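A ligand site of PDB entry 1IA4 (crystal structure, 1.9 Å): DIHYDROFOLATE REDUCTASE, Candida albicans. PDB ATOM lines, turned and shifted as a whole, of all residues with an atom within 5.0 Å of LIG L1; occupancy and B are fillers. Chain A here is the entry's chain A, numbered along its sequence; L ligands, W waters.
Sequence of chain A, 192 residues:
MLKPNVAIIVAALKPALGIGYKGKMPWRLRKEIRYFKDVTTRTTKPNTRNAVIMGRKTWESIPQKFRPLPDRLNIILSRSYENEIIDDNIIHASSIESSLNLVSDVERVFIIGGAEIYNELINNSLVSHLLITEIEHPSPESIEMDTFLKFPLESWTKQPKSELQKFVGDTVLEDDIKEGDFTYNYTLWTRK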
ATOM      1  N   ILE A   9     -27.904  17.775 -20.318  1.00  0.00           N
ATOM      2  CA  ILE A   9     -26.934  16.765 -19.766  1.00  0.00           C
ATOM      3  C   ILE A   9     -27.072  15.551 -20.622  1.00  0.00           C
ATOM      4  O   ILE A   9     -28.189  14.976 -20.841  1.00  0.00           O
ATOM      5  CB  ILE A   9     -27.188  16.556 -18.237  1.00  0.00           C
ATOM      6  CG1 ILE A   9     -26.182  15.477 -17.684  1.00  0.00           C
ATOM      7  CG2 ILE A   9     -28.625  16.118 -17.903  1.00  0.00           C
ATOM      8  CD1 ILE A   9     -26.146  15.438 -16.135  1.00  0.00           C
ATOM      9  N   VAL A  10     -25.959  15.117 -21.198  1.00  0.00           N
ATOM     10  CA  VAL A  10     -25.927  13.977 -22.133  1.00  0.00           C
ATOM     11  C   VAL A  10     -24.615  13.177 -22.033  1.00  0.00           C
ATOM     12  O   VAL A  10     -23.619  13.750 -21.572  1.00  0.00           O
ATOM     13  CB  VAL A  10     -26.018  14.582 -23.558  1.00  0.00           C
ATOM     14  CG1 VAL A  10     -24.958  15.637 -23.810  1.00  0.00           C
ATOM     15  CG2 VAL A  10     -26.124  13.578 -24.666  1.00  0.00           C
ATOM     16  N   ALA A  11     -24.634  11.977 -22.520  1.00  0.00           N
ATOM     17  CA  ALA A  11     -23.482  11.088 -22.552  1.00  0.00           C
ATOM     18  C   ALA A  11     -23.276  10.789 -24.035  1.00  0.00           C
ATOM     19  O   ALA A  11     -24.260  10.374 -24.687  1.00  0.00           O
ATOM     20  CB  ALA A  11     -23.709   9.847 -21.723  1.00  0.00           C
ATOM     21  N   ILE A  19     -25.024   8.795 -29.571  1.00  0.00           N
ATOM     22  CA  ILE A  19     -25.769   8.816 -28.311  1.00  0.00           C
ATOM     23  C   ILE A  19     -26.755   7.676 -28.150  1.00  0.00           C
ATOM     24  O   ILE A  19     -27.269   7.470 -27.049  1.00  0.00           O
ATOM     25  CB  ILE A  19     -26.487  10.177 -28.059  1.00  0.00           C
ATOM     26  CG1 ILE A  19     -27.347  10.545 -29.341  1.00  0.00           C
ATOM     27  CG2 ILE A  19     -25.530  11.332 -27.710  1.00  0.00           C
ATOM     28  CD1 ILE A  19     -28.253  11.846 -29.008  1.00  0.00           C
ATOM     29  N   GLY A  20     -27.005   6.964 -29.250  1.00  0.00           N
ATOM     30  CA  GLY A  20     -27.961   5.850 -29.151  1.00  0.00           C
ATOM     31  C   GLY A  20     -28.019   4.985 -30.380  1.00  0.00           C
ATOM     32  O   GLY A  20     -27.447   5.247 -31.453  1.00  0.00           O
ATOM     33  N   GLY A  23     -33.132   3.645 -30.068  1.00  0.00           N
ATOM     34  CA  GLY A  23     -33.797   4.006 -28.820  1.00  0.00           C
ATOM     35  C   GLY A  23     -33.115   3.712 -27.527  1.00  0.00           C
ATOM     36  O   GLY A  23     -33.720   4.018 -26.444  1.00  0.00           O
ATOM     37  N   LYS A  24     -31.907   3.154 -27.587  1.00  0.00           N
ATOM     38  CA  LYS A  24     -31.144   2.823 -26.369  1.00  0.00           C
ATOM     39  C   LYS A  24     -29.714   3.271 -26.416  1.00  0.00           C
ATOM     40  O   LYS A  24     -29.081   3.351 -27.492  1.00  0.00           O
ATOM     41  CB  LYS A  24     -31.272   1.347 -26.019  1.00  0.00           C
ATOM     42  CG  LYS A  24     -30.930   0.233 -26.944  1.00  0.00           C
ATOM     43  CD  LYS A  24     -29.531   0.219 -27.539  1.00  0.00           C
ATOM     44  CE  LYS A  24     -28.885  -1.119 -27.806  1.00  0.00           C
ATOM     45  NZ  LYS A  24     -28.401  -1.633 -26.451  1.00  0.00           N
ATOM     46  N   MET A  25     -29.166   3.537 -25.235  1.00  0.00           N
ATOM     47  CA  MET A  25     -27.711   3.925 -25.152  1.00  0.00           C
ATOM     48  C   MET A  25     -26.965   2.602 -25.431  1.00  0.00           C
ATOM     49  O   MET A  25     -27.347   1.564 -24.848  1.00  0.00           O
ATOM     50  CB  MET A  25     -27.380   4.429 -23.762  1.00  0.00           C
ATOM     51  CG  MET A  25     -28.248   5.526 -23.256  1.00  0.00           C
ATOM     52  SD  MET A  25     -27.661   6.068 -21.618  1.00  0.00           S
ATOM     53  CE  MET A  25     -26.439   7.256 -22.045  1.00  0.00           C
ATOM     54  N   GLU A  32     -21.657   6.261 -14.384  1.00  0.00           N
ATOM     55  CA  GLU A  32     -22.160   7.413 -15.148  1.00  0.00           C
ATOM     56  C   GLU A  32     -23.643   7.631 -14.803  1.00  0.00           C
ATOM     57  O   GLU A  32     -24.044   8.782 -14.615  1.00  0.00           O
ATOM     58  CB  GLU A  32     -22.014   7.189 -16.652  1.00  0.00           C
ATOM     59  CG  GLU A  32     -21.791   8.492 -17.497  1.00  0.00           C
ATOM     60  CD  GLU A  32     -23.118   9.260 -17.689  1.00  0.00           C
ATOM     61  OE1 GLU A  32     -24.161   8.659 -17.818  1.00  0.00           O
ATOM     62  OE2 GLU A  32     -22.973  10.473 -17.706  1.00  0.00           O
ATOM     63  N   ILE A  33     -24.401   6.552 -14.698  1.00  0.00           N
ATOM     64  CA  ILE A  33     -25.845   6.701 -14.335  1.00  0.00           C
ATOM     65  C   ILE A  33     -25.977   7.297 -12.940  1.00  0.00           C
ATOM     66  O   ILE A  33     -26.876   8.051 -12.661  1.00  0.00           O
ATOM     67  CB  ILE A  33     -26.620   5.345 -14.394  1.00  0.00           C
ATOM     68  CG1 ILE A  33     -26.388   4.601 -15.675  1.00  0.00           C
ATOM     69  CG2 ILE A  33     -28.144   5.559 -14.032  1.00  0.00           C
ATOM     70  CD1 ILE A  33     -26.875   4.989 -17.025  1.00  0.00           C
ATOM     71  N   TYR A  35     -23.831   9.402 -11.418  1.00  0.00           N
ATOM     72  CA  TYR A  35     -23.504  10.839 -11.571  1.00  0.00           C
ATOM     73  C   TYR A  35     -24.794  11.572 -12.139  1.00  0.00           C
ATOM     74  O   TYR A  35     -25.114  12.626 -11.572  1.00  0.00           O
ATOM     75  CB  TYR A  35     -22.447  10.959 -12.670  1.00  0.00           C
ATOM     76  CG  TYR A  35     -22.154  12.350 -13.186  1.00  0.00           C
ATOM     77  CD1 TYR A  35     -22.691  12.845 -14.377  1.00  0.00           C
ATOM     78  CD2 TYR A  35     -21.366  13.189 -12.401  1.00  0.00           C
ATOM     79  CE1 TYR A  35     -22.381  14.144 -14.803  1.00  0.00           C
ATOM     80  CE2 TYR A  35     -20.988  14.457 -12.835  1.00  0.00           C
ATOM     81  CZ  TYR A  35     -21.534  14.941 -14.026  1.00  0.00           C
ATOM     82  OH  TYR A  35     -21.167  16.190 -14.360  1.00  0.00           O
ATOM     83  N   PHE A  36     -25.358  11.015 -13.170  1.00  0.00           N
ATOM     84  CA  PHE A  36     -26.629  11.647 -13.742  1.00  0.00           C
ATOM     85  C   PHE A  36     -27.608  11.841 -12.597  1.00  0.00           C
ATOM     86  O   PHE A  36     -28.253  12.908 -12.473  1.00  0.00           O
ATOM     87  CB  PHE A  36     -27.176  10.852 -14.928  1.00  0.00           C
ATOM     88  CG  PHE A  36     -28.583  11.226 -15.364  1.00  0.00           C
ATOM     89  CD1 PHE A  36     -29.661  10.526 -14.821  1.00  0.00           C
ATOM     90  CD2 PHE A  36     -28.816  12.394 -16.150  1.00  0.00           C
ATOM     91  CE1 PHE A  36     -30.992  10.864 -15.138  1.00  0.00           C
ATOM     92  CE2 PHE A  36     -30.173  12.698 -16.482  1.00  0.00           C
ATOM     93  CZ  PHE A  36     -31.215  11.970 -15.978  1.00  0.00           C
ATOM     94  N   THR A  58     -38.861   9.590 -24.815  1.00  0.00           N
ATOM     95  CA  THR A  58     -38.011   9.148 -23.672  1.00  0.00           C
ATOM     96  C   THR A  58     -38.928   8.815 -22.500  1.00  0.00           C
ATOM     97  O   THR A  58     -38.740   7.778 -21.887  1.00  0.00           O
ATOM     98  CB  THR A  58     -36.987  10.277 -23.285  1.00  0.00           C
ATOM     99  OG1 THR A  58     -36.153  10.486 -24.455  1.00  0.00           O
ATOM    100  CG2 THR A  58     -36.219  10.023 -22.020  1.00  0.00           C
ATOM    101  N   ILE A 112     -32.866  16.396 -20.374  1.00  0.00           N
ATOM    102  CA  ILE A 112     -32.308  15.042 -20.299  1.00  0.00           C
ATOM    103  C   ILE A 112     -32.376  14.227 -21.526  1.00  0.00           C
ATOM    104  O   ILE A 112     -31.569  13.222 -21.605  1.00  0.00           O
ATOM    105  CB  ILE A 112     -32.810  14.290 -18.989  1.00  0.00           C
ATOM    106  CG1 ILE A 112     -34.240  13.814 -19.093  1.00  0.00           C
ATOM    107  CG2 ILE A 112     -32.531  15.200 -17.740  1.00  0.00           C
ATOM    108  CD1 ILE A 112     -34.797  12.833 -18.006  1.00  0.00           C
ATOM    109  N   GLY A 113     -33.109  14.654 -22.573  1.00  0.00           N
ATOM    110  CA  GLY A 113     -33.120  13.801 -23.778  1.00  0.00           C
ATOM    111  C   GLY A 113     -34.577  13.810 -24.351  1.00  0.00           C
ATOM    112  O   GLY A 113     -35.401  14.415 -23.651  1.00  0.00           O
ATOM    113  N   GLY A 114     -34.822  13.139 -25.439  1.00  0.00           N
ATOM    114  CA  GLY A 114     -33.850  12.381 -26.222  1.00  0.00           C
ATOM    115  C   GLY A 114     -33.185  13.139 -27.319  1.00  0.00           C
ATOM    116  O   GLY A 114     -33.035  14.355 -27.238  1.00  0.00           O
ATOM    117  N   ALA A 115     -32.811  12.407 -28.390  1.00  0.00           N
ATOM    118  CA  ALA A 115     -32.099  12.947 -29.524  1.00  0.00           C
ATOM    119  C   ALA A 115     -32.761  14.167 -30.169  1.00  0.00           C
ATOM    120  O   ALA A 115     -32.043  15.159 -30.421  1.00  0.00           O
ATOM    121  CB  ALA A 115     -31.947  11.911 -30.599  1.00  0.00           C
ATOM    122  N   TYR A 118     -32.535  17.166 -27.764  1.00  0.00           N
ATOM    123  CA  TYR A 118     -31.181  17.674 -27.720  1.00  0.00           C
ATOM    124  C   TYR A 118     -30.880  18.576 -28.911  1.00  0.00           C
ATOM    125  O   TYR A 118     -30.388  19.667 -28.687  1.00  0.00           O
ATOM    126  CB  TYR A 118     -30.066  16.584 -27.669  1.00  0.00           C
ATOM    127  CG  TYR A 118     -29.975  15.704 -26.450  1.00  0.00           C
ATOM    128  CD1 TYR A 118     -30.098  16.192 -25.133  1.00  0.00           C
ATOM    129  CD2 TYR A 118     -29.676  14.356 -26.617  1.00  0.00           C
ATOM    130  CE1 TYR A 118     -29.903  15.359 -24.026  1.00  0.00           C
ATOM    131  CE2 TYR A 118     -29.499  13.509 -25.536  1.00  0.00           C
ATOM    132  CZ  TYR A 118     -29.587  14.023 -24.246  1.00  0.00           C
ATOM    133  OH  TYR A 118     -29.455  13.134 -23.201  1.00  0.00           O
ATOM    134  N   LEU A 131     -23.541  19.709 -20.073  1.00  0.00           N
ATOM    135  CA  LEU A 131     -22.793  18.732 -19.197  1.00  0.00           C
ATOM    136  C   LEU A 131     -22.739  17.476 -20.095  1.00  0.00           C
ATOM    137  O   LEU A 131     -23.690  16.743 -20.184  1.00  0.00           O
ATOM    138  CB  LEU A 131     -23.482  18.517 -17.882  1.00  0.00           C
ATOM    139  CG  LEU A 131     -23.563  19.670 -16.901  1.00  0.00           C
ATOM    140  CD1 LEU A 131     -24.753  19.468 -15.950  1.00  0.00           C
ATOM    141  CD2 LEU A 131     -22.273  19.778 -16.086  1.00  0.00           C
ATOM    142  N   THR A 133     -20.828  14.020 -20.944  1.00  0.00           N
ATOM    143  CA  THR A 133     -19.847  12.951 -20.486  1.00  0.00           C
ATOM    144  C   THR A 133     -19.194  12.464 -21.798  1.00  0.00           C
ATOM    145  O   THR A 133     -19.920  11.956 -22.680  1.00  0.00           O
ATOM    146  CB  THR A 133     -20.577  11.760 -19.776  1.00  0.00           C
ATOM    147  OG1 THR A 133     -21.226  12.329 -18.615  1.00  0.00           O
ATOM    148  CG2 THR A 133     -19.562  10.639 -19.358  1.00  0.00           C
ATOM    149  N   THR A 147     -27.905   7.349 -33.900  1.00  0.00           N
ATOM    150  CA  THR A 147     -28.325   8.708 -33.440  1.00  0.00           C
ATOM    151  C   THR A 147     -27.159   9.500 -32.980  1.00  0.00           C
ATOM    152  O   THR A 147     -26.242   8.920 -32.359  1.00  0.00           O
ATOM    153  CB  THR A 147     -29.297   8.339 -32.220  1.00  0.00           C
ATOM    154  OG1 THR A 147     -30.297   7.429 -32.817  1.00  0.00           O
ATOM    155  CG2 THR A 147     -29.918   9.544 -31.650  1.00  0.00           C
HETATM  156  C1  LIG L   1     -28.246  11.691 -19.495  1.00  0.00           C
HETATM  157  N1  LIG L   1     -27.050  12.234 -19.425  1.00  0.00           N
HETATM  158  C2  LIG L   1     -26.027  11.595 -18.835  1.00  0.00           C
HETATM  159  N2  LIG L   1     -26.132  10.298 -18.428  1.00  0.00           N
HETATM  160  C3  LIG L   1     -29.875   8.319 -18.540  1.00  0.00           C
HETATM  161  C4  LIG L   1     -29.753   9.615 -19.036  1.00  0.00           C
HETATM  162  C5  LIG L   1     -28.552  10.342 -19.000  1.00  0.00           C
HETATM  163  C6  LIG L   1     -27.432   9.621 -18.492  1.00  0.00           C
HETATM  164  C7  LIG L   1     -27.567   8.355 -17.948  1.00  0.00           C
HETATM  165  C8  LIG L   1     -28.767   7.661 -17.995  1.00  0.00           C
HETATM  166  N3  LIG L   1     -24.830  12.171 -18.777  1.00  0.00           N
HETATM  167  N4  LIG L   1     -29.069  12.573 -20.043  1.00  0.00           N
HETATM  168  S1  LIG L   1     -31.281  10.333 -19.610  1.00  0.00           S
HETATM  169  C9  LIG L   1     -31.177   9.879 -21.338  1.00  0.00           C
HETATM  170  C10 LIG L   1     -30.018   9.583 -22.052  1.00  0.00           C
HETATM  171  C11 LIG L   1     -29.990   9.247 -23.385  1.00  0.00           C
HETATM  172  C12 LIG L   1     -31.205   9.235 -24.179  1.00  0.00           C
HETATM  173  C13 LIG L   1     -32.341   9.565 -23.485  1.00  0.00           C
HETATM  174  C14 LIG L   1     -32.363   9.839 -22.119  1.00  0.00           C
HETATM  175  C15 LIG L   1     -31.730   8.959 -27.905  1.00  0.00           C
HETATM  176  C16 LIG L   1     -31.001   9.431 -26.691  1.00  0.00           C
HETATM  177  N5  LIG L   1     -31.179   8.784 -25.437  1.00  0.00           N
HETATM  178  C17 LIG L   1     -31.626   7.308 -25.532  1.00  0.00           C
HETATM  179  C18 LIG L   1     -31.378   6.878 -26.980  1.00  0.00           C
HETATM  180  O1  LIG L   1     -32.299   7.683 -27.744  1.00  0.00           O
HETATM  181  P1  LG2 L   2     -37.295  12.264 -27.689  1.00  0.00           P
HETATM  182  O1  LG2 L   2     -36.417  13.360 -28.058  1.00  0.00           O
HETATM  183  O2  LG2 L   2     -37.265  11.857 -26.266  1.00  0.00           O
HETATM  184  O3  LG2 L   2     -38.856  12.685 -28.012  1.00  0.00           O
HETATM  185  C1  LG2 L   2     -39.159  13.322 -29.272  1.00  0.00           C
HETATM  186  C2  LG2 L   2     -40.616  13.812 -29.090  1.00  0.00           C
HETATM  187  O4  LG2 L   2     -40.558  14.952 -28.247  1.00  0.00           O
HETATM  188  C3  LG2 L   2     -41.185  14.396 -30.434  1.00  0.00           C
HETATM  189  O5  LG2 L   2     -41.553  13.240 -31.174  1.00  0.00           O
HETATM  190  C4  LG2 L   2     -42.328  15.280 -29.803  1.00  0.00           C
HETATM  191  O6  LG2 L   2     -43.395  14.591 -29.122  1.00  0.00           O
HETATM  192  C5  LG2 L   2     -41.572  15.868 -28.621  1.00  0.00           C
HETATM  193  N1  LG2 L   2     -40.888  17.039 -28.995  1.00  0.00           N
HETATM  194  C6  LG2 L   2     -39.699  16.950 -29.675  1.00  0.00           C
HETATM  195  N2  LG2 L   2     -39.211  18.127 -29.956  1.00  0.00           N
HETATM  196  C7  LG2 L   2     -40.121  18.990 -29.388  1.00  0.00           C
HETATM  197  C8  LG2 L   2     -40.110  20.391 -29.410  1.00  0.00           C
HETATM  198  N3  LG2 L   2     -39.089  21.067 -29.993  1.00  0.00           N
HETATM  199  N4  LG2 L   2     -41.142  20.982 -28.761  1.00  0.00           N
HETATM  200  C9  LG2 L   2     -42.159  20.181 -28.285  1.00  0.00           C
HETATM  201  N5  LG2 L   2     -42.253  18.882 -28.263  1.00  0.00           N
HETATM  202  C10 LG2 L   2     -41.155  18.330 -28.810  1.00  0.00           C
HETATM  203  O7  LG2 L   2     -37.108  11.037 -28.573  1.00  0.00           O
HETATM  204  P2  LG2 L   2     -35.971  10.464 -29.607  1.00  0.00           P
HETATM  205  O8  LG2 L   2     -34.797  10.104 -28.747  1.00  0.00           O
HETATM  206  O9  LG2 L   2     -35.670  11.485 -30.599  1.00  0.00           O
HETATM  207  O10 LG2 L   2     -36.631   9.155 -30.162  1.00  0.00           O
HETATM  208  C11 LG2 L   2     -35.934   7.976 -30.596  1.00  0.00           C
HETATM  209  C12 LG2 L   2     -36.750   7.061 -31.495  1.00  0.00           C
HETATM  210  O11 LG2 L   2     -36.002   6.774 -32.711  1.00  0.00           O
HETATM  211  C13 LG2 L   2     -37.223   5.732 -30.916  1.00  0.00           C
HETATM  212  P3  LG2 L   2     -44.784  14.385 -30.089  1.00  0.00           P
HETATM  213  O12 LG2 L   2     -45.589  13.689 -29.009  1.00  0.00           O
HETATM  214  O13 LG2 L   2     -44.964  15.742 -30.525  1.00  0.00           O
HETATM  215  O14 LG2 L   2     -44.332  13.428 -31.108  1.00  0.00           O
HETATM  216  O   HOH W   1     -27.112  10.772 -22.870  1.00  0.00           O
HETATM  217  O   HOH W   2     -22.614  14.605 -18.330  1.00  0.00           O
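Residues that only touch LIG L1: Ala 11 (3.8 Å), Gly 23 (3.7 Å), Lys 24 (3.8 Å), Ile 33 (3.4 Å), Phe 36 (3.5 Å), Thr 58 (3.9 Å), Ala 115 (3.6 Å) and Thr 133 (3.6 Å).
Hydrophobic or aromatic side chains that line LIG L1: Ile 9, Ala 11, Ile 33 and Phe 36.
Within 4 Å of LIG L1: Ile 9, Val 10, Ala 11, Gly 23, Lys 24, Glu 32, Ile 33, Phe 36, Thr 58, Ile 112, Ala 115, Tyr 118 and Thr 133.
The nearest printed residue that does not touch LIG L1 is Met 25 (4.1 Å).
OE1 of Glu 32 is in hydrogen-bond range of N2 of LIG L1, at 2.6 Å.
N4 of LIG L1 is in hydrogen-bond range of O of Ile 9 (2.7 Å).
The backbone carbonyl oxygen of Ile 112 sits at hydrogen-bond distance from a nitrogen (N4) of LIG L1, 3.0 Å away.
A nitrogen (N4) of LIG L1 lies within hydrogen-bond range of the side-chain hydroxyl (OH) of Tyr 118, 3.2 Å away.
A nitrogen (N3) of LIG L1 sits close to the backbone carbonyl oxygen (O) of Val 10 (3.4 Å).
An oxygen (O8) of LG2 L2 sits at hydrogen-bond distance from the backbone NH (N) of Ala 115 (3.1 Å).
N of Thr 58 sits at hydrogen-bond distance from O2 of LG2 L2.
OG1 of Thr 58 sits at hydrogen-bond distance from O2 of LG2 L2, 2.5 Å away.
An oxygen (O2) of LG2 L2 lies within hydrogen-bond range of the backbone NH of Gly 114, at 2.9 Å.
Water W1 lies within hydrogen-bond range of N of Ala 11 and OH of Tyr 118.
Water W2 lies within hydrogen-bond range of OG1 of Thr 133, O of Leu 131 and N3 of LIG L1.
The side-chain carboxylate (OE2) of Glu 32 is in hydrogen-bond range of the side-chain hydroxyl (OG1) of Thr 133, 2.7 Å away.
O of Ile 9 lies within hydrogen-bond range of OH of Tyr 118 (3.3 Å).
O of Ile 112 lies within hydrogen-bond range of OH of Tyr 118 (2.7 Å).
The backbone carbonyl oxygen (O) of Val 10 sits at hydrogen-bond distance from the backbone NH (N) of Thr 133.
The backbone carbonyl oxygen (O) of Leu 131 is in hydrogen-bond range of the backbone NH (N) of Val 10 (3.0 Å).
The backbone NH of Gly 114 lies within hydrogen-bond range of the side-chain hydroxyl of Thr 58 (3.1 Å).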
